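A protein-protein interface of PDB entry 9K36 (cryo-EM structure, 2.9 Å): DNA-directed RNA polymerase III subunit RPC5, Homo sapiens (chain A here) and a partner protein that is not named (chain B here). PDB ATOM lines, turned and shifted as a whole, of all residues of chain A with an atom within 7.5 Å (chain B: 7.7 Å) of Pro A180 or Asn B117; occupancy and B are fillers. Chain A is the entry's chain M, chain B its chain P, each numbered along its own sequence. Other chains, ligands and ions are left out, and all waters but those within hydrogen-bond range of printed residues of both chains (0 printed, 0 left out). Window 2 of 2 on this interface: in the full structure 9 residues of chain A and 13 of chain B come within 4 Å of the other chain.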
ATOM      1  N   PHE A 177       7.545 -23.596   3.386  1.00  0.00           N
ATOM      2  CA  PHE A 177       7.968 -22.685   4.439  1.00  0.00           C
ATOM      3  C   PHE A 177       8.803 -21.554   3.860  1.00  0.00           C
ATOM      4  O   PHE A 177       9.760 -21.790   3.116  1.00  0.00           O
ATOM      5  CB  PHE A 177       8.779 -23.435   5.499  1.00  0.00           C
ATOM      6  CG  PHE A 177       7.944 -24.196   6.486  1.00  0.00           C
ATOM      7  CD1 PHE A 177       6.562 -24.130   6.448  1.00  0.00           C
ATOM      8  CD2 PHE A 177       8.547 -24.968   7.465  1.00  0.00           C
ATOM      9  CE1 PHE A 177       5.801 -24.829   7.363  1.00  0.00           C
ATOM     10  CE2 PHE A 177       7.792 -25.666   8.381  1.00  0.00           C
ATOM     11  CZ  PHE A 177       6.418 -25.595   8.335  1.00  0.00           C
ATOM     12  N   SER A 178       8.443 -20.319   4.205  1.00  0.00           N
ATOM     13  CA  SER A 178       9.295 -19.167   3.915  1.00  0.00           C
ATOM     14  C   SER A 178      10.433 -19.191   4.928  1.00  0.00           C
ATOM     15  O   SER A 178      10.471 -18.429   5.897  1.00  0.00           O
ATOM     16  CB  SER A 178       8.500 -17.868   3.975  1.00  0.00           C
ATOM     17  OG  SER A 178       7.979 -17.649   5.274  1.00  0.00           O
ATOM     18  N   ARG A 179      11.368 -20.111   4.702  1.00  0.00           N
ATOM     19  CA  ARG A 179      12.444 -20.349   5.654  1.00  0.00           C
ATOM     20  C   ARG A 179      13.280 -19.087   5.834  1.00  0.00           C
ATOM     21  O   ARG A 179      13.562 -18.392   4.848  1.00  0.00           O
ATOM     22  CB  ARG A 179      13.338 -21.495   5.181  1.00  0.00           C
ATOM     23  CG  ARG A 179      12.630 -22.823   4.977  1.00  0.00           C
ATOM     24  CD  ARG A 179      13.614 -23.890   4.526  1.00  0.00           C
ATOM     25  NE  ARG A 179      12.973 -25.183   4.307  1.00  0.00           N
ATOM     26  CZ  ARG A 179      13.617 -26.277   3.909  1.00  0.00           C
ATOM     27  NH1 ARG A 179      14.924 -26.235   3.687  1.00  0.00           N
ATOM     28  NH2 ARG A 179      12.954 -27.411   3.732  1.00  0.00           N
ATOM     29  N   PRO A 180      13.684 -18.752   7.058  1.00  0.00           N
ATOM     30  CA  PRO A 180      14.620 -17.637   7.235  1.00  0.00           C
ATOM     31  C   PRO A 180      15.956 -17.954   6.587  1.00  0.00           C
ATOM     32  O   PRO A 180      16.700 -18.823   7.060  1.00  0.00           O
ATOM     33  CB  PRO A 180      14.737 -17.509   8.759  1.00  0.00           C
ATOM     34  CG  PRO A 180      14.362 -18.859   9.283  1.00  0.00           C
ATOM     35  CD  PRO A 180      13.323 -19.387   8.337  1.00  0.00           C
ATOM     36  N   GLU A 181      16.267 -17.256   5.501  1.00  0.00           N
ATOM     37  CA  GLU A 181      17.450 -17.585   4.719  1.00  0.00           C
ATOM     38  C   GLU A 181      18.707 -17.065   5.404  1.00  0.00           C
ATOM     39  O   GLU A 181      18.742 -15.934   5.898  1.00  0.00           O
ATOM     40  CB  GLU A 181      17.331 -16.996   3.314  1.00  0.00           C
ATOM     41  CG  GLU A 181      18.355 -17.531   2.329  1.00  0.00           C
ATOM     42  CD  GLU A 181      18.191 -16.940   0.944  1.00  0.00           C
ATOM     43  OE1 GLU A 181      17.498 -15.909   0.815  1.00  0.00           O
ATOM     44  OE2 GLU A 181      18.755 -17.504  -0.018  1.00  0.00           O
ATOM     45  N   SER A 182      19.736 -17.907   5.442  1.00  0.00           N
ATOM     46  CA  SER A 182      21.020 -17.489   5.985  1.00  0.00           C
ATOM     47  C   SER A 182      21.573 -16.323   5.177  1.00  0.00           C
ATOM     48  O   SER A 182      21.344 -16.220   3.969  1.00  0.00           O
ATOM     49  CB  SER A 182      22.008 -18.659   5.982  1.00  0.00           C
ATOM     50  OG  SER A 182      22.213 -19.152   4.671  1.00  0.00           O
ATOM     51  N   GLU A 183      22.298 -15.432   5.860  1.00  0.00           N
ATOM     52  CA  GLU A 183      22.796 -14.226   5.207  1.00  0.00           C
ATOM     53  C   GLU A 183      23.695 -14.553   4.022  1.00  0.00           C
ATOM     54  O   GLU A 183      23.673 -13.841   3.012  1.00  0.00           O
ATOM     55  CB  GLU A 183      23.532 -13.349   6.220  1.00  0.00           C
ATOM     56  CG  GLU A 183      23.809 -11.937   5.733  1.00  0.00           C
ATOM     57  CD  GLU A 183      24.239 -11.011   6.854  1.00  0.00           C
ATOM     58  OE1 GLU A 183      24.426 -11.497   7.991  1.00  0.00           O
ATOM     59  OE2 GLU A 183      24.382  -9.796   6.602  1.00  0.00           O
ATOM     60  N   ALA A 185      23.423 -17.288   2.070  1.00  0.00           N
ATOM     61  CA  ALA A 185      22.539 -17.727   0.993  1.00  0.00           C
ATOM     62  C   ALA A 185      21.727 -16.564   0.439  1.00  0.00           C
ATOM     63  O   ALA A 185      21.439 -16.518  -0.763  1.00  0.00           O
ATOM     64  CB  ALA A 185      21.622 -18.843   1.487  1.00  0.00           C
ATOM     65  N   GLN B  91       5.239 -17.337  12.586  1.00  0.00           N
ATOM     66  CA  GLN B  91       5.938 -18.600  12.803  1.00  0.00           C
ATOM     67  C   GLN B  91       4.974 -19.716  13.193  1.00  0.00           C
ATOM     68  O   GLN B  91       5.196 -20.883  12.841  1.00  0.00           O
ATOM     69  CB  GLN B  91       7.018 -18.431  13.874  1.00  0.00           C
ATOM     70  CG  GLN B  91       8.317 -17.816  13.365  1.00  0.00           C
ATOM     71  CD  GLN B  91       8.152 -16.385  12.884  1.00  0.00           C
ATOM     72  OE1 GLN B  91       7.226 -15.683  13.290  1.00  0.00           O
ATOM     73  NE2 GLN B  91       9.054 -15.947  12.012  1.00  0.00           N
ATOM     74  N   LEU B  94       3.724 -20.796   9.974  1.00  0.00           N
ATOM     75  CA  LEU B  94       4.883 -21.292   9.245  1.00  0.00           C
ATOM     76  C   LEU B  94       5.496 -22.531   9.886  1.00  0.00           C
ATOM     77  O   LEU B  94       6.592 -22.936   9.495  1.00  0.00           O
ATOM     78  CB  LEU B  94       5.937 -20.186   9.136  1.00  0.00           C
ATOM     79  CG  LEU B  94       6.910 -20.237   7.958  1.00  0.00           C
ATOM     80  CD1 LEU B  94       6.164 -20.050   6.647  1.00  0.00           C
ATOM     81  CD2 LEU B  94       8.001 -19.190   8.119  1.00  0.00           C
ATOM     82  N   ARG B 110      13.207 -33.479  14.227  1.00  0.00           N
ATOM     83  CA  ARG B 110      14.375 -33.140  13.420  1.00  0.00           C
ATOM     84  C   ARG B 110      13.968 -32.664  12.030  1.00  0.00           C
ATOM     85  O   ARG B 110      14.500 -31.669  11.525  1.00  0.00           O
ATOM     86  CB  ARG B 110      15.309 -34.346  13.316  1.00  0.00           C
ATOM     87  CG  ARG B 110      16.530 -34.110  12.445  1.00  0.00           C
ATOM     88  CD  ARG B 110      17.095 -35.423  11.921  1.00  0.00           C
ATOM     89  NE  ARG B 110      17.441 -36.347  12.996  1.00  0.00           N
ATOM     90  CZ  ARG B 110      18.665 -36.486  13.496  1.00  0.00           C
ATOM     91  NH1 ARG B 110      19.666 -35.763  13.018  1.00  0.00           N
ATOM     92  NH2 ARG B 110      18.886 -37.353  14.477  1.00  0.00           N
ATOM     93  N   ASP B 111      13.026 -33.367  11.396  1.00  0.00           N
ATOM     94  CA  ASP B 111      12.581 -32.969  10.066  1.00  0.00           C
ATOM     95  C   ASP B 111      11.825 -31.650  10.109  1.00  0.00           C
ATOM     96  O   ASP B 111      11.936 -30.834   9.185  1.00  0.00           O
ATOM     97  CB  ASP B 111      11.718 -34.072   9.451  1.00  0.00           C
ATOM     98  CG  ASP B 111      12.443 -35.398   9.364  1.00  0.00           C
ATOM     99  OD1 ASP B 111      13.682 -35.393   9.213  1.00  0.00           O
ATOM    100  OD2 ASP B 111      11.771 -36.448   9.449  1.00  0.00           O
ATOM    101  N   ILE B 112      11.052 -31.416  11.171  1.00  0.00           N
ATOM    102  CA  ILE B 112      10.375 -30.130  11.328  1.00  0.00           C
ATOM    103  C   ILE B 112      11.395 -29.006  11.448  1.00  0.00           C
ATOM    104  O   ILE B 112      11.254 -27.946  10.826  1.00  0.00           O
ATOM    105  CB  ILE B 112       9.426 -30.163  12.542  1.00  0.00           C
ATOM    106  CG1 ILE B 112       8.344 -31.225  12.351  1.00  0.00           C
ATOM    107  CG2 ILE B 112       8.789 -28.802  12.758  1.00  0.00           C
ATOM    108  CD1 ILE B 112       7.393 -31.342  13.521  1.00  0.00           C
ATOM    109  N   ARG B 113      12.445 -29.223  12.245  1.00  0.00           N
ATOM    110  CA  ARG B 113      13.493 -28.220  12.388  1.00  0.00           C
ATOM    111  C   ARG B 113      14.207 -27.969  11.064  1.00  0.00           C
ATOM    112  O   ARG B 113      14.517 -26.820  10.726  1.00  0.00           O
ATOM    113  CB  ARG B 113      14.490 -28.659  13.460  1.00  0.00           C
ATOM    114  CG  ARG B 113      15.777 -27.855  13.492  1.00  0.00           C
ATOM    115  CD  ARG B 113      16.779 -28.463  14.460  1.00  0.00           C
ATOM    116  NE  ARG B 113      18.069 -27.783  14.412  1.00  0.00           N
ATOM    117  CZ  ARG B 113      19.132 -28.148  15.123  1.00  0.00           C
ATOM    118  NH1 ARG B 113      19.058 -29.190  15.940  1.00  0.00           N
ATOM    119  NH2 ARG B 113      20.266 -27.471  15.016  1.00  0.00           N
ATOM    120  N   TYR B 114      14.469 -29.033  10.299  1.00  0.00           N
ATOM    121  CA  TYR B 114      15.187 -28.871   9.040  1.00  0.00           C
ATOM    122  C   TYR B 114      14.330 -28.173   7.989  1.00  0.00           C
ATOM    123  O   TYR B 114      14.843 -27.381   7.189  1.00  0.00           O
ATOM    124  CB  TYR B 114      15.667 -30.230   8.528  1.00  0.00           C
ATOM    125  CG  TYR B 114      16.900 -30.748   9.235  1.00  0.00           C
ATOM    126  CD1 TYR B 114      17.732 -29.889   9.940  1.00  0.00           C
ATOM    127  CD2 TYR B 114      17.233 -32.096   9.193  1.00  0.00           C
ATOM    128  CE1 TYR B 114      18.860 -30.356  10.586  1.00  0.00           C
ATOM    129  CE2 TYR B 114      18.359 -32.573   9.836  1.00  0.00           C
ATOM    130  CZ  TYR B 114      19.167 -31.698  10.531  1.00  0.00           C
ATOM    131  OH  TYR B 114      20.290 -32.171  11.173  1.00  0.00           O
ATOM    132  N   LYS B 115      13.024 -28.450   7.972  1.00  0.00           N
ATOM    133  CA  LYS B 115      12.150 -27.796   7.003  1.00  0.00           C
ATOM    134  C   LYS B 115      11.837 -26.361   7.409  1.00  0.00           C
ATOM    135  O   LYS B 115      11.570 -25.520   6.543  1.00  0.00           O
ATOM    136  CB  LYS B 115      10.858 -28.593   6.829  1.00  0.00           C
ATOM    137  CG  LYS B 115      11.021 -29.911   6.080  1.00  0.00           C
ATOM    138  CD  LYS B 115       9.666 -30.549   5.810  1.00  0.00           C
ATOM    139  CE  LYS B 115       9.797 -31.865   5.053  1.00  0.00           C
ATOM    140  NZ  LYS B 115      10.498 -32.902   5.860  1.00  0.00           N
ATOM    141  N   SER B 116      11.865 -26.061   8.706  1.00  0.00           N
ATOM    142  CA  SER B 116      11.594 -24.711   9.183  1.00  0.00           C
ATOM    143  C   SER B 116      12.831 -23.821   9.206  1.00  0.00           C
ATOM    144  O   SER B 116      12.689 -22.599   9.319  1.00  0.00           O
ATOM    145  CB  SER B 116      10.979 -24.762  10.585  1.00  0.00           C
ATOM    146  OG  SER B 116      11.855 -25.392  11.502  1.00  0.00           O
ATOM    147  N   ASN B 117      14.028 -24.404   9.093  1.00  0.00           N
ATOM    148  CA  ASN B 117      15.286 -23.653   9.107  1.00  0.00           C
ATOM    149  C   ASN B 117      15.386 -22.758  10.343  1.00  0.00           C
ATOM    150  O   ASN B 117      15.841 -21.616  10.274  1.00  0.00           O
ATOM    151  CB  ASN B 117      15.459 -22.835   7.824  1.00  0.00           C
ATOM    152  CG  ASN B 117      16.917 -22.547   7.498  1.00  0.00           C
ATOM    153  OD1 ASN B 117      17.767 -22.495   8.386  1.00  0.00           O
ATOM    154  ND2 ASN B 117      17.212 -22.356   6.216  1.00  0.00           N
ATOM    155  N   LEU B 118      14.953 -23.286  11.481  1.00  0.00           N
ATOM    156  CA  LEU B 118      14.964 -22.587  12.756  1.00  0.00           C
ATOM    157  C   LEU B 118      15.741 -23.402  13.772  1.00  0.00           C
ATOM    158  O   LEU B 118      15.835 -24.630  13.656  1.00  0.00           O
ATOM    159  CB  LEU B 118      13.537 -22.339  13.266  1.00  0.00           C
ATOM    160  CG  LEU B 118      12.699 -21.313  12.507  1.00  0.00           C
ATOM    161  CD1 LEU B 118      11.274 -21.297  13.031  1.00  0.00           C
ATOM    162  CD2 LEU B 118      13.328 -19.933  12.611  1.00  0.00           C
ATOM    163  N   PRO B 119      16.317 -22.754  14.781  1.00  0.00           N
ATOM    164  CA  PRO B 119      17.028 -23.494  15.830  1.00  0.00           C
ATOM    165  C   PRO B 119      16.077 -24.377  16.627  1.00  0.00           C
ATOM    166  O   PRO B 119      14.854 -24.304  16.509  1.00  0.00           O
ATOM    167  CB  PRO B 119      17.639 -22.392  16.701  1.00  0.00           C
ATOM    168  CG  PRO B 119      17.700 -21.192  15.807  1.00  0.00           C
ATOM    169  CD  PRO B 119      16.493 -21.298  14.923  1.00  0.00           C
ATOM    170  N   LEU B 120      16.676 -25.231  17.461  1.00  0.00           N
ATOM    171  CA  LEU B 120      15.895 -26.225  18.190  1.00  0.00           C
ATOM    172  C   LEU B 120      15.022 -25.578  19.261  1.00  0.00           C
ATOM    173  O   LEU B 120      13.913 -26.047  19.533  1.00  0.00           O
ATOM    174  CB  LEU B 120      16.830 -27.266  18.808  1.00  0.00           C
ATOM    175  CG  LEU B 120      16.177 -28.496  19.436  1.00  0.00           C
ATOM    176  CD1 LEU B 120      15.318 -29.232  18.420  1.00  0.00           C
ATOM    177  CD2 LEU B 120      17.240 -29.419  20.013  1.00  0.00           C
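The guanidinium group (NE) of Arg A179 is in hydrogen-bond range of the backbone carbonyl oxygen (O) of Lys B115, 2.7 Å away.
The backbone carbonyl oxygen of Ile B112 is in hydrogen-bond range of the side-chain hydroxyl of Ser B116, 2.7 Å away. OG of Ser B116 sits at hydrogen-bond distance from O of Arg B113, 3.1 Å away.
Among the printed residues, pairs that only touch across the chains: Phe A177 with Leu B94 (2.9 Å), Phe A177 with Lys B115 (3.2 Å), Ser A178 with Leu B94 (3.2 Å), Pro A180 with Asn B117 (3.3 Å), Pro A180 with Ser B116 (3.4 Å), Phe A177 with Ser B116 (3.5 Å), Arg A179 with Asn B117 (3.6 Å), Pro A180 with Leu B118 (3.6 Å) and Arg A179 with Tyr B114 (3.7 Å).
Of chain B, only Ser B116, Asn B117 and Leu B118 come within 4 Å of Pro A180. Printed residues of chain A within 4 Å of Asn B117: Arg A179 (3.6 Å) and Pro A180 (3.3 Å). Printed residues of chain A within 4 Å of Ser B116: Phe A177 (3.5 Å) and Pro A180 (3.4 Å). Printed residues of chain A within 4 Å of Lys B115: Phe A177 (3.2 Å) and Arg A179 (2.7 Å). Of the printed residues of chain A, Leu B94 touches Phe A177 (2.9 Å) and Ser A178 (3.2 Å). Of the printed residues of chain B, Arg A179 touches Tyr B114 (3.7 Å), Lys B115 (2.7 Å) and Asn B117 (3.6 Å). Of the printed residues of chain B, Ser A178 touches Leu B94 (3.2 Å). Printed residues of chain A within 4 Å of Leu B118: Pro A180 (3.6 Å). The nearest residue of chain A that does not touch Asn B117 is Glu A181 (5.0 Å).
Printed residues of chain B that touch a printed residue of chain A: Leu B94, Tyr B114, Lys B115, Ser B116, Asn B117 and Leu B118. Hydrophobic or aromatic side chains of chain A that line the printed part of chain B: Phe A177 and Pro A180. Among the printed residues, no Asp or Glu carboxylate lies within 4 Å of a Lys or Arg side-chain nitrogen of the other chain.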
